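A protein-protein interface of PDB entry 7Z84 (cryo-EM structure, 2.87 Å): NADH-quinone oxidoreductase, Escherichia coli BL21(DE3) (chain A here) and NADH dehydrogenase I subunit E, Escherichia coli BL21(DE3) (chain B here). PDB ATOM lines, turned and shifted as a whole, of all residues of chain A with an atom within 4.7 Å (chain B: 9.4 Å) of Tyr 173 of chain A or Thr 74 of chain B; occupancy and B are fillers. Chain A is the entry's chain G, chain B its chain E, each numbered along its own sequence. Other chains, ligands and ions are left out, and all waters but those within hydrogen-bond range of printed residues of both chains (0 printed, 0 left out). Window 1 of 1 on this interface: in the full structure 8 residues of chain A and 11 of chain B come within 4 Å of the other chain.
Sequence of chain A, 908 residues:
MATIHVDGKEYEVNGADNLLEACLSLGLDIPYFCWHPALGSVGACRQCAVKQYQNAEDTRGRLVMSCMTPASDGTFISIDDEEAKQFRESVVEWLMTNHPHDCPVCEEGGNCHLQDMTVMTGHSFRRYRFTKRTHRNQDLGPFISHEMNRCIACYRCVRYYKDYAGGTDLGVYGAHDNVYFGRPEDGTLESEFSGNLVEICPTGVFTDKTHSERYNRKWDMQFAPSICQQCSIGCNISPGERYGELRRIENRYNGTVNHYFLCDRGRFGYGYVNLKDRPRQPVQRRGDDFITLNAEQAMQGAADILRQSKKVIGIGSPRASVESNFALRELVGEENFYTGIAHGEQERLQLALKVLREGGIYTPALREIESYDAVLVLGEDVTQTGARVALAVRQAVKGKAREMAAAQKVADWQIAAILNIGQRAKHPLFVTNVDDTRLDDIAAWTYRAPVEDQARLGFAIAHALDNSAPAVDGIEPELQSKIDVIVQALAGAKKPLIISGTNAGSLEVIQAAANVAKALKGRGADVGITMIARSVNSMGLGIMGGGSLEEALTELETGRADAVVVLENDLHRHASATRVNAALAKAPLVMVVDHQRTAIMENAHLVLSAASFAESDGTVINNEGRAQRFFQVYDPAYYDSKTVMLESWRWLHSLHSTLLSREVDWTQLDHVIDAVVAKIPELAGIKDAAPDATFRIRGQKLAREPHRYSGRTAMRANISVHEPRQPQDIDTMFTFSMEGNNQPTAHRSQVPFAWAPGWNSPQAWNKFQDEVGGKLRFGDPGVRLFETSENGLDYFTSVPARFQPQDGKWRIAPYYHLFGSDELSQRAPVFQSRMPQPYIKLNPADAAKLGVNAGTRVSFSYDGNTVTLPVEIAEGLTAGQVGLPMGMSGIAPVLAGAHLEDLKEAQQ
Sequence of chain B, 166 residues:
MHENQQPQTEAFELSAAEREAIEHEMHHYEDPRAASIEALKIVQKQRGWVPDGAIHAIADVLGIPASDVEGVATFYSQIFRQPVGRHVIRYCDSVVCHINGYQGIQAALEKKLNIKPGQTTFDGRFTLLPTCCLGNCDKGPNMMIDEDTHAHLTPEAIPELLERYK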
ATOM      1  N   ASP A 169      13.734 -12.223 -16.760  1.00  0.00           N
ATOM      2  CA  ASP A 169      13.244 -12.576 -15.435  1.00  0.00           C
ATOM      3  C   ASP A 169      14.049 -11.967 -14.293  1.00  0.00           C
ATOM      4  O   ASP A 169      13.749 -12.253 -13.133  1.00  0.00           O
ATOM      5  CB  ASP A 169      13.203 -14.098 -15.278  1.00  0.00           C
ATOM      6  CG  ASP A 169      14.491 -14.762 -15.702  1.00  0.00           C
ATOM      7  OD1 ASP A 169      15.123 -14.280 -16.660  1.00  0.00           O
ATOM      8  OD2 ASP A 169      14.870 -15.770 -15.076  1.00  0.00           O
ATOM      9  N   LEU A 170      15.052 -11.144 -14.578  1.00  0.00           N
ATOM     10  CA  LEU A 170      15.784 -10.427 -13.543  1.00  0.00           C
ATOM     11  C   LEU A 170      15.514  -8.936 -13.670  1.00  0.00           C
ATOM     12  O   LEU A 170      15.491  -8.391 -14.778  1.00  0.00           O
ATOM     13  CB  LEU A 170      17.288 -10.689 -13.631  1.00  0.00           C
ATOM     14  CG  LEU A 170      18.142 -10.294 -12.425  1.00  0.00           C
ATOM     15  CD1 LEU A 170      18.353 -11.482 -11.507  1.00  0.00           C
ATOM     16  CD2 LEU A 170      19.469  -9.708 -12.867  1.00  0.00           C
ATOM     17  N   GLY A 171      15.318  -8.279 -12.532  1.00  0.00           N
ATOM     18  CA  GLY A 171      14.995  -6.868 -12.535  1.00  0.00           C
ATOM     19  C   GLY A 171      15.252  -6.234 -11.186  1.00  0.00           C
ATOM     20  O   GLY A 171      15.635  -6.896 -10.216  1.00  0.00           O
ATOM     21  N   VAL A 172      15.036  -4.922 -11.149  1.00  0.00           N
ATOM     22  CA  VAL A 172      15.175  -4.113  -9.945  1.00  0.00           C
ATOM     23  C   VAL A 172      13.780  -3.725  -9.468  1.00  0.00           C
ATOM     24  O   VAL A 172      12.913  -3.363 -10.272  1.00  0.00           O
ATOM     25  CB  VAL A 172      16.075  -2.884 -10.191  1.00  0.00           C
ATOM     26  CG1 VAL A 172      15.583  -2.042 -11.364  1.00  0.00           C
ATOM     27  CG2 VAL A 172      16.196  -2.035  -8.933  1.00  0.00           C
ATOM     28  N   TYR A 173      13.550  -3.858  -8.166  1.00  0.00           N
ATOM     29  CA  TYR A 173      12.256  -3.612  -7.554  1.00  0.00           C
ATOM     30  C   TYR A 173      12.443  -2.718  -6.344  1.00  0.00           C
ATOM     31  O   TYR A 173      13.519  -2.678  -5.744  1.00  0.00           O
ATOM     32  CB  TYR A 173      11.585  -4.920  -7.126  1.00  0.00           C
ATOM     33  CG  TYR A 173      11.828  -6.034  -8.101  1.00  0.00           C
ATOM     34  CD1 TYR A 173      11.147  -6.089  -9.307  1.00  0.00           C
ATOM     35  CD2 TYR A 173      12.764  -7.016  -7.829  1.00  0.00           C
ATOM     36  CE1 TYR A 173      11.381  -7.098 -10.207  1.00  0.00           C
ATOM     37  CE2 TYR A 173      13.002  -8.025  -8.717  1.00  0.00           C
ATOM     38  CZ  TYR A 173      12.310  -8.064  -9.907  1.00  0.00           C
ATOM     39  OH  TYR A 173      12.553  -9.074 -10.801  1.00  0.00           O
ATOM     40  N   GLY A 174      11.390  -1.998  -5.988  1.00  0.00           N
ATOM     41  CA  GLY A 174      11.432  -1.225  -4.769  1.00  0.00           C
ATOM     42  C   GLY A 174      11.792   0.233  -4.942  1.00  0.00           C
ATOM     43  O   GLY A 174      11.509   0.843  -5.975  1.00  0.00           O
ATOM     44  N   ALA A 175      12.442   0.789  -3.927  1.00  0.00           N
ATOM     45  CA  ALA A 175      12.486   2.231  -3.742  1.00  0.00           C
ATOM     46  C   ALA A 175      13.791   2.672  -3.096  1.00  0.00           C
ATOM     47  O   ALA A 175      14.790   1.949  -3.138  1.00  0.00           O
ATOM     48  CB  ALA A 175      11.294   2.698  -2.906  1.00  0.00           C
ATOM     49  N   ASN A 178      15.669   0.604  -0.307  1.00  0.00           N
ATOM     50  CA  ASN A 178      15.240  -0.786  -0.297  1.00  0.00           C
ATOM     51  C   ASN A 178      15.194  -1.380  -1.700  1.00  0.00           C
ATOM     52  O   ASN A 178      14.287  -2.160  -2.010  1.00  0.00           O
ATOM     53  CB  ASN A 178      13.874  -0.908   0.375  1.00  0.00           C
ATOM     54  CG  ASN A 178      13.790  -2.092   1.312  1.00  0.00           C
ATOM     55  OD1 ASN A 178      14.760  -2.435   1.986  1.00  0.00           O
ATOM     56  ND2 ASN A 178      12.628  -2.728   1.356  1.00  0.00           N
ATOM     57  N   VAL A 179      16.141  -1.008  -2.563  1.00  0.00           N
ATOM     58  CA  VAL A 179      16.198  -1.576  -3.906  1.00  0.00           C
ATOM     59  C   VAL A 179      16.587  -3.044  -3.825  1.00  0.00           C
ATOM     60  O   VAL A 179      17.551  -3.417  -3.144  1.00  0.00           O
ATOM     61  CB  VAL A 179      17.173  -0.790  -4.793  1.00  0.00           C
ATOM     62  CG1 VAL A 179      16.500   0.427  -5.377  1.00  0.00           C
ATOM     63  CG2 VAL A 179      18.388  -0.368  -3.994  1.00  0.00           C
ATOM     64  N   TYR A 180      15.828  -3.884  -4.516  1.00  0.00           N
ATOM     65  CA  TYR A 180      16.043  -5.321  -4.553  1.00  0.00           C
ATOM     66  C   TYR A 180      16.361  -5.718  -5.983  1.00  0.00           C
ATOM     67  O   TYR A 180      15.729  -5.224  -6.920  1.00  0.00           O
ATOM     68  CB  TYR A 180      14.807  -6.064  -4.045  1.00  0.00           C
ATOM     69  CG  TYR A 180      15.073  -7.464  -3.560  1.00  0.00           C
ATOM     70  CD1 TYR A 180      15.006  -8.544  -4.428  1.00  0.00           C
ATOM     71  CD2 TYR A 180      15.381  -7.708  -2.232  1.00  0.00           C
ATOM     72  CE1 TYR A 180      15.245  -9.826  -3.987  1.00  0.00           C
ATOM     73  CE2 TYR A 180      15.621  -8.984  -1.781  1.00  0.00           C
ATOM     74  CZ  TYR A 180      15.551 -10.040  -2.662  1.00  0.00           C
ATOM     75  OH  TYR A 180      15.789 -11.316  -2.214  1.00  0.00           O
ATOM     76  N   GLY A 182      16.707  -9.008  -8.428  1.00  0.00           N
ATOM     77  CA  GLY A 182      16.469 -10.436  -8.514  1.00  0.00           C
ATOM     78  C   GLY A 182      15.273 -10.746  -9.388  1.00  0.00           C
ATOM     79  O   GLY A 182      14.895  -9.957 -10.250  1.00  0.00           O
ATOM     80  N   ARG A 183      14.714 -11.913  -9.170  1.00  0.00           N
ATOM     81  CA  ARG A 183      13.523 -12.351  -9.875  1.00  0.00           C
ATOM     82  C   ARG A 183      12.272 -11.862  -9.158  1.00  0.00           C
ATOM     83  O   ARG A 183      12.305 -11.584  -7.956  1.00  0.00           O
ATOM     84  CB  ARG A 183      13.521 -13.873  -9.981  1.00  0.00           C
ATOM     85  CG  ARG A 183      14.713 -14.438 -10.722  1.00  0.00           C
ATOM     86  CD  ARG A 183      14.542 -15.922 -10.954  1.00  0.00           C
ATOM     87  NE  ARG A 183      13.804 -16.195 -12.181  1.00  0.00           N
ATOM     88  CZ  ARG A 183      12.542 -16.599 -12.220  1.00  0.00           C
ATOM     89  NH1 ARG A 183      11.840 -16.780 -11.114  1.00  0.00           N
ATOM     90  NH2 ARG A 183      11.970 -16.824 -13.398  1.00  0.00           N
ATOM     91  N   PRO A 184      11.144 -11.722  -9.870  1.00  0.00           N
ATOM     92  CA  PRO A 184       9.892 -11.361  -9.181  1.00  0.00           C
ATOM     93  C   PRO A 184       9.391 -12.433  -8.229  1.00  0.00           C
ATOM     94  O   PRO A 184       8.589 -12.122  -7.341  1.00  0.00           O
ATOM     95  CB  PRO A 184       8.905 -11.133 -10.333  1.00  0.00           C
ATOM     96  CG  PRO A 184       9.477 -11.874 -11.482  1.00  0.00           C
ATOM     97  CD  PRO A 184      10.958 -11.798 -11.331  1.00  0.00           C
ATOM     98  N   ILE B  37       1.625   1.540 -15.764  1.00  0.00           N
ATOM     99  CA  ILE B  37       1.178   2.221 -14.552  1.00  0.00           C
ATOM    100  C   ILE B  37      -0.342   2.301 -14.512  1.00  0.00           C
ATOM    101  O   ILE B  37      -0.970   2.003 -13.489  1.00  0.00           O
ATOM    102  CB  ILE B  37       1.823   3.616 -14.463  1.00  0.00           C
ATOM    103  CG1 ILE B  37       3.338   3.493 -14.300  1.00  0.00           C
ATOM    104  CG2 ILE B  37       1.224   4.425 -13.327  1.00  0.00           C
ATOM    105  CD1 ILE B  37       4.070   4.794 -14.468  1.00  0.00           C
ATOM    106  N   LEU B  40      -1.866  -1.201 -13.916  1.00  0.00           N
ATOM    107  CA  LEU B  40      -1.800  -1.528 -12.496  1.00  0.00           C
ATOM    108  C   LEU B  40      -2.830  -0.737 -11.704  1.00  0.00           C
ATOM    109  O   LEU B  40      -3.437  -1.263 -10.766  1.00  0.00           O
ATOM    110  CB  LEU B  40      -0.396  -1.262 -11.955  1.00  0.00           C
ATOM    111  CG  LEU B  40       0.742  -2.171 -12.417  1.00  0.00           C
ATOM    112  CD1 LEU B  40       2.073  -1.487 -12.192  1.00  0.00           C
ATOM    113  CD2 LEU B  40       0.701  -3.489 -11.683  1.00  0.00           C
ATOM    114  N   VAL B  50      -3.003  -4.918  -5.989  1.00  0.00           N
ATOM    115  CA  VAL B  50      -2.475  -5.654  -7.135  1.00  0.00           C
ATOM    116  C   VAL B  50      -1.927  -6.996  -6.662  1.00  0.00           C
ATOM    117  O   VAL B  50      -0.847  -7.044  -6.059  1.00  0.00           O
ATOM    118  CB  VAL B  50      -1.394  -4.845  -7.868  1.00  0.00           C
ATOM    119  CG1 VAL B  50      -0.932  -5.586  -9.105  1.00  0.00           C
ATOM    120  CG2 VAL B  50      -1.920  -3.469  -8.234  1.00  0.00           C
ATOM    121  N   ILE B  55       0.493  -9.195 -11.973  1.00  0.00           N
ATOM    122  CA  ILE B  55       1.725  -8.772 -12.634  1.00  0.00           C
ATOM    123  C   ILE B  55       1.933  -9.559 -13.921  1.00  0.00           C
ATOM    124  O   ILE B  55       2.210  -8.988 -14.983  1.00  0.00           O
ATOM    125  CB  ILE B  55       2.922  -8.927 -11.678  1.00  0.00           C
ATOM    126  CG1 ILE B  55       2.709  -8.087 -10.416  1.00  0.00           C
ATOM    127  CG2 ILE B  55       4.220  -8.546 -12.370  1.00  0.00           C
ATOM    128  CD1 ILE B  55       2.702  -6.598 -10.664  1.00  0.00           C
ATOM    129  N   HIS B  56       1.763 -10.882 -13.852  1.00  0.00           N
ATOM    130  CA  HIS B  56       1.932 -11.716 -15.038  1.00  0.00           C
ATOM    131  C   HIS B  56       0.813 -11.487 -16.047  1.00  0.00           C
ATOM    132  O   HIS B  56       1.053 -11.538 -17.257  1.00  0.00           O
ATOM    133  CB  HIS B  56       2.007 -13.189 -14.643  1.00  0.00           C
ATOM    134  CG  HIS B  56       3.243 -13.545 -13.881  1.00  0.00           C
ATOM    135  ND1 HIS B  56       3.485 -13.093 -12.602  1.00  0.00           N
ATOM    136  CD2 HIS B  56       4.313 -14.301 -14.222  1.00  0.00           C
ATOM    137  CE1 HIS B  56       4.648 -13.559 -12.186  1.00  0.00           C
ATOM    138  NE2 HIS B  56       5.171 -14.295 -13.149  1.00  0.00           N
ATOM    139  N   PRO B  65       8.142  -7.888 -20.205  1.00  0.00           N
ATOM    140  CA  PRO B  65       8.444  -8.867 -19.152  1.00  0.00           C
ATOM    141  C   PRO B  65       7.801  -8.513 -17.818  1.00  0.00           C
ATOM    142  O   PRO B  65       7.586  -7.344 -17.493  1.00  0.00           O
ATOM    143  CB  PRO B  65       9.971  -8.821 -19.056  1.00  0.00           C
ATOM    144  CG  PRO B  65      10.410  -8.421 -20.406  1.00  0.00           C
ATOM    145  CD  PRO B  65       9.355  -7.498 -20.947  1.00  0.00           C
ATOM    146  N   ALA B  66       7.495  -9.556 -17.040  1.00  0.00           N
ATOM    147  CA  ALA B  66       6.864  -9.380 -15.736  1.00  0.00           C
ATOM    148  C   ALA B  66       7.787  -8.728 -14.718  1.00  0.00           C
ATOM    149  O   ALA B  66       7.298  -8.161 -13.736  1.00  0.00           O
ATOM    150  CB  ALA B  66       6.377 -10.728 -15.203  1.00  0.00           C
ATOM    151  N   SER B  67       9.105  -8.808 -14.924  1.00  0.00           N
ATOM    152  CA  SER B  67      10.043  -8.167 -14.008  1.00  0.00           C
ATOM    153  C   SER B  67       9.898  -6.650 -14.037  1.00  0.00           C
ATOM    154  O   SER B  67       9.964  -5.998 -12.990  1.00  0.00           O
ATOM    155  CB  SER B  67      11.473  -8.580 -14.350  1.00  0.00           C
ATOM    156  OG  SER B  67      11.758  -8.346 -15.716  1.00  0.00           O
ATOM    157  N   ASP B  68       9.680  -6.074 -15.222  1.00  0.00           N
ATOM    158  CA  ASP B  68       9.489  -4.629 -15.319  1.00  0.00           C
ATOM    159  C   ASP B  68       8.170  -4.195 -14.693  1.00  0.00           C
ATOM    160  O   ASP B  68       8.103  -3.139 -14.054  1.00  0.00           O
ATOM    161  CB  ASP B  68       9.562  -4.183 -16.777  1.00  0.00           C
ATOM    162  CG  ASP B  68      10.652  -4.889 -17.546  1.00  0.00           C
ATOM    163  OD1 ASP B  68      10.333  -5.543 -18.556  1.00  0.00           O
ATOM    164  OD2 ASP B  68      11.828  -4.794 -17.139  1.00  0.00           O
ATOM    165  N   VAL B  69       7.116  -4.998 -14.857  1.00  0.00           N
ATOM    166  CA  VAL B  69       5.834  -4.692 -14.230  1.00  0.00           C
ATOM    167  C   VAL B  69       5.948  -4.766 -12.712  1.00  0.00           C
ATOM    168  O   VAL B  69       5.400  -3.922 -11.995  1.00  0.00           O
ATOM    169  CB  VAL B  69       4.738  -5.633 -14.760  1.00  0.00           C
ATOM    170  CG1 VAL B  69       3.364  -5.141 -14.335  1.00  0.00           C
ATOM    171  CG2 VAL B  69       4.823  -5.740 -16.267  1.00  0.00           C
ATOM    172  N   GLU B  70       6.663  -5.773 -12.200  1.00  0.00           N
ATOM    173  CA  GLU B  70       6.871  -5.885 -10.761  1.00  0.00           C
ATOM    174  C   GLU B  70       7.718  -4.732 -10.231  1.00  0.00           C
ATOM    175  O   GLU B  70       7.448  -4.207  -9.144  1.00  0.00           O
ATOM    176  CB  GLU B  70       7.520  -7.229 -10.433  1.00  0.00           C
ATOM    177  CG  GLU B  70       7.799  -7.458  -8.956  1.00  0.00           C
ATOM    178  CD  GLU B  70       6.536  -7.668  -8.147  1.00  0.00           C
ATOM    179  OE1 GLU B  70       5.564  -8.227  -8.694  1.00  0.00           O
ATOM    180  OE2 GLU B  70       6.515  -7.274  -6.963  1.00  0.00           O
ATOM    181  N   GLY B  71       8.734  -4.318 -10.991  1.00  0.00           N
ATOM    182  CA  GLY B  71       9.546  -3.184 -10.578  1.00  0.00           C
ATOM    183  C   GLY B  71       8.775  -1.879 -10.573  1.00  0.00           C
ATOM    184  O   GLY B  71       8.976  -1.036  -9.695  1.00  0.00           O
ATOM    185  N   VAL B  72       7.883  -1.696 -11.547  1.00  0.00           N
ATOM    186  CA  VAL B  72       7.025  -0.516 -11.560  1.00  0.00           C
ATOM    187  C   VAL B  72       6.052  -0.549 -10.386  1.00  0.00           C
ATOM    188  O   VAL B  72       5.872   0.455  -9.689  1.00  0.00           O
ATOM    189  CB  VAL B  72       6.301  -0.404 -12.914  1.00  0.00           C
ATOM    190  CG1 VAL B  72       5.130   0.556 -12.830  1.00  0.00           C
ATOM    191  CG2 VAL B  72       7.270   0.052 -13.986  1.00  0.00           C
ATOM    192  N   ALA B  73       5.439  -1.707 -10.125  1.00  0.00           N
ATOM    193  CA  ALA B  73       4.471  -1.815  -9.037  1.00  0.00           C
ATOM    194  C   ALA B  73       5.124  -1.596  -7.676  1.00  0.00           C
ATOM    195  O   ALA B  73       4.521  -0.987  -6.786  1.00  0.00           O
ATOM    196  CB  ALA B  73       3.776  -3.173  -9.086  1.00  0.00           C
ATOM    197  N   THR B  74       6.352  -2.083  -7.494  1.00  0.00           N
ATOM    198  CA  THR B  74       7.060  -1.867  -6.241  1.00  0.00           C
ATOM    199  C   THR B  74       7.717  -0.495  -6.159  1.00  0.00           C
ATOM    200  O   THR B  74       8.062  -0.057  -5.056  1.00  0.00           O
ATOM    201  CB  THR B  74       8.120  -2.948  -6.044  1.00  0.00           C
ATOM    202  OG1 THR B  74       8.859  -3.111  -7.259  1.00  0.00           O
ATOM    203  CG2 THR B  74       7.470  -4.267  -5.674  1.00  0.00           C
ATOM    204  N   PHE B  75       7.904   0.188  -7.290  1.00  0.00           N
ATOM    205  CA  PHE B  75       8.494   1.522  -7.256  1.00  0.00           C
ATOM    206  C   PHE B  75       7.511   2.549  -6.711  1.00  0.00           C
ATOM    207  O   PHE B  75       7.866   3.374  -5.862  1.00  0.00           O
ATOM    208  CB  PHE B  75       8.966   1.924  -8.654  1.00  0.00           C
ATOM    209  CG  PHE B  75       9.748   3.207  -8.686  1.00  0.00           C
ATOM    210  CD1 PHE B  75      11.104   3.213  -8.411  1.00  0.00           C
ATOM    211  CD2 PHE B  75       9.129   4.408  -8.997  1.00  0.00           C
ATOM    212  CE1 PHE B  75      11.826   4.386  -8.443  1.00  0.00           C
ATOM    213  CE2 PHE B  75       9.846   5.584  -9.025  1.00  0.00           C
ATOM    214  CZ  PHE B  75      11.196   5.574  -8.749  1.00  0.00           C
ATOM    215  N   TYR B  76       6.271   2.512  -7.185  1.00  0.00           N
ATOM    216  CA  TYR B  76       5.311   3.572  -6.916  1.00  0.00           C
ATOM    217  C   TYR B  76       4.557   3.280  -5.627  1.00  0.00           C
ATOM    218  O   TYR B  76       4.089   2.158  -5.412  1.00  0.00           O
ATOM    219  CB  TYR B  76       4.345   3.721  -8.092  1.00  0.00           C
ATOM    220  CG  TYR B  76       5.016   4.260  -9.333  1.00  0.00           C
ATOM    221  CD1 TYR B  76       5.298   5.610  -9.464  1.00  0.00           C
ATOM    222  CD2 TYR B  76       5.385   3.414 -10.365  1.00  0.00           C
ATOM    223  CE1 TYR B  76       5.920   6.097 -10.596  1.00  0.00           C
ATOM    224  CE2 TYR B  76       6.008   3.889 -11.493  1.00  0.00           C
ATOM    225  CZ  TYR B  76       6.274   5.231 -11.604  1.00  0.00           C
ATOM    226  OH  TYR B  76       6.894   5.702 -12.733  1.00  0.00           O
ATOM    227  N   SER B  77       4.446   4.298  -4.772  1.00  0.00           N
ATOM    228  CA  SER B  77       3.864   4.100  -3.450  1.00  0.00           C
ATOM    229  C   SER B  77       2.354   3.915  -3.507  1.00  0.00           C
ATOM    230  O   SER B  77       1.783   3.252  -2.634  1.00  0.00           O
ATOM    231  CB  SER B  77       4.221   5.277  -2.544  1.00  0.00           C
ATOM    232  OG  SER B  77       3.814   6.503  -3.121  1.00  0.00           O
ATOM    233  N   GLN B  78       1.690   4.479  -4.513  1.00  0.00           N
ATOM    234  CA  GLN B  78       0.240   4.392  -4.609  1.00  0.00           C
ATOM    235  C   GLN B  78      -0.237   3.124  -5.301  1.00  0.00           C
ATOM    236  O   GLN B  78      -1.449   2.920  -5.418  1.00  0.00           O
ATOM    237  CB  GLN B  78      -0.323   5.616  -5.337  1.00  0.00           C
ATOM    238  CG  GLN B  78      -0.352   6.902  -4.514  1.00  0.00           C
ATOM    239  CD  GLN B  78      -0.311   6.667  -3.015  1.00  0.00           C
ATOM    240  OE1 GLN B  78      -1.294   6.229  -2.413  1.00  0.00           O
ATOM    241  NE2 GLN B  78       0.829   6.962  -2.403  1.00  0.00           N
ATOM    242  N   ILE B  79       0.672   2.276  -5.767  1.00  0.00           N
ATOM    243  CA  ILE B  79       0.328   0.952  -6.271  1.00  0.00           C
ATOM    244  C   ILE B  79       0.641  -0.035  -5.158  1.00  0.00           C
ATOM    245  O   ILE B  79       1.806  -0.233  -4.797  1.00  0.00           O
ATOM    246  CB  ILE B  79       1.091   0.611  -7.557  1.00  0.00           C
ATOM    247  CG1 ILE B  79       0.661   1.536  -8.695  1.00  0.00           C
ATOM    248  CG2 ILE B  79       0.858  -0.841  -7.941  1.00  0.00           C
ATOM    249  CD1 ILE B  79       1.611   1.532  -9.867  1.00  0.00           C
ATOM    250  N   PHE B  80      -0.396  -0.657  -4.609  1.00  0.00           N
ATOM    251  CA  PHE B  80      -0.258  -1.501  -3.432  1.00  0.00           C
ATOM    252  C   PHE B  80      -0.085  -2.952  -3.864  1.00  0.00           C
ATOM    253  O   PHE B  80      -0.954  -3.511  -4.541  1.00  0.00           O
ATOM    254  CB  PHE B  80      -1.471  -1.346  -2.518  1.00  0.00           C
ATOM    255  CG  PHE B  80      -1.788   0.079  -2.171  1.00  0.00           C
ATOM    256  CD1 PHE B  80      -0.786   0.948  -1.772  1.00  0.00           C
ATOM    257  CD2 PHE B  80      -3.085   0.554  -2.252  1.00  0.00           C
ATOM    258  CE1 PHE B  80      -1.073   2.262  -1.456  1.00  0.00           C
ATOM    259  CE2 PHE B  80      -3.379   1.867  -1.936  1.00  0.00           C
ATOM    260  CZ  PHE B  80      -2.371   2.721  -1.539  1.00  0.00           C
ATOM    261  N   ARG B  81       1.036  -3.552  -3.476  1.00  0.00           N
ATOM    262  CA  ARG B  81       1.314  -4.953  -3.750  1.00  0.00           C
ATOM    263  C   ARG B  81       1.035  -5.842  -2.546  1.00  0.00           C
ATOM    264  O   ARG B  81       1.358  -7.033  -2.576  1.00  0.00           O
ATOM    265  CB  ARG B  81       2.761  -5.120  -4.212  1.00  0.00           C
ATOM    266  CG  ARG B  81       2.978  -4.796  -5.677  1.00  0.00           C
ATOM    267  CD  ARG B  81       2.224  -5.765  -6.564  1.00  0.00           C
ATOM    268  NE  ARG B  81       2.988  -6.982  -6.804  1.00  0.00           N
ATOM    269  CZ  ARG B  81       2.673  -8.173  -6.316  1.00  0.00           C
ATOM    270  NH1 ARG B  81       1.608  -8.347  -5.551  1.00  0.00           N
ATOM    271  NH2 ARG B  81       3.446  -9.216  -6.601  1.00  0.00           N
ATOM    272  N   GLN B  82       0.450  -5.286  -1.492  1.00  0.00           N
ATOM    273  CA  GLN B  82      -0.007  -6.010  -0.319  1.00  0.00           C
ATOM    274  C   GLN B  82      -1.464  -5.658  -0.066  1.00  0.00           C
ATOM    275  O   GLN B  82      -1.896  -4.547  -0.389  1.00  0.00           O
ATOM    276  CB  GLN B  82       0.841  -5.662   0.914  1.00  0.00           C
ATOM    277  CG  GLN B  82       1.780  -6.776   1.344  1.00  0.00           C
ATOM    278  CD  GLN B  82       2.985  -6.263   2.101  1.00  0.00           C
ATOM    279  OE1 GLN B  82       2.900  -5.280   2.835  1.00  0.00           O
ATOM    280  NE2 GLN B  82       4.120  -6.931   1.928  1.00  0.00           N
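Hydrophobic or aromatic side chains of chain B that line the printed part of chain A: Phe 75. Along chain A the printed residues that touch a printed residue of chain B span positions 170 to 174. Among the printed residues, no Asp or Glu carboxylate lies within 4 Å of a Lys or Arg side-chain nitrogen of the other chain.
The side-chain hydroxyl (OG1) of Thr 74 of chain B is in hydrogen-bond range of the backbone NH (N) of Gly 174 of chain A, 3.0 Å away.
Printed residues of chain B within 4 Å of Leu 170 of chain A: Ser 67 (3.8 Å). No residue of chain B comes within 4 Å of Gly 171 of chain A. Of chain B, only Gly 71 comes within 4 Å of Val 172 of chain A. Of chain B, only Ser 67, Glu 70, Gly 71 and Thr 74 come within 4 Å of Tyr 173 of chain A. Gly 174 of chain A touches just these residues of chain B: Thr 74 and Phe 75. Of the printed residues of chain A, Ser 67 of chain B touches Leu 170 and Tyr 173. Printed residues of chain A within 4 Å of Glu 70 of chain B: Tyr 173 (3.6 Å). Val 72 of chain B touches none of the printed residues of chain A. Thr 74 of chain B touches just these residues of chain A: Tyr 173 and Gly 174. The nearest residue of chain B that does not touch Tyr 173 of chain A is Asp 68 of chain B (5.4 Å). The nearest printed residue of chain B that does not touch Leu 170 of chain A is Asp 68 of chain B (5.7 Å).
Ser 67 of chain B touches Leu 170 of chain A (OG to O, 3.8 Å). Val 172 of chain A touches Gly 71 of chain B (O to CA, 3.4 Å). O of Ser 67 of chain B touches CE1 of Tyr 173 of chain A, 3.3 Å away. Tyr 173 of chain A touches Glu 70 of chain B (CD1 to CG, 3.6 Å). Tyr 173 of chain A touches Gly 71 of chain B. Tyr 173 of chain A touches Thr 74 of chain B. Gly 174 of chain A touches Phe 75 of chain B.
The backbone NH (N) of Tyr 173 of chain A sits at hydrogen-bond distance from the backbone carbonyl oxygen (O) of Tyr 180 of chain A, 2.9 Å away. The backbone NH (N) of Gly 171 of chain A lies within hydrogen-bond range of the side-chain hydroxyl (OH) of Tyr 173 of chain A (3.4 Å). The side-chain carboxylate of Glu 70 of chain B lies within salt-bridge range of the guanidinium group of Arg 81 of chain B, at 3.1 Å. The side-chain hydroxyl (OH) of Tyr 173 of chain A lies within hydrogen-bond range of the backbone carbonyl oxygen (O) of Gly 182 of chain A, 2.6 Å away. The backbone carbonyl oxygen (O) of Gly 71 of chain B sits at hydrogen-bond distance from the side-chain hydroxyl (OG1) of Thr 74 of chain B (3.2 Å). The backbone carbonyl oxygen of Glu 70 of chain B lies within hydrogen-bond range of the side-chain hydroxyl of Thr 74 of chain B, at 2.6 Å.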
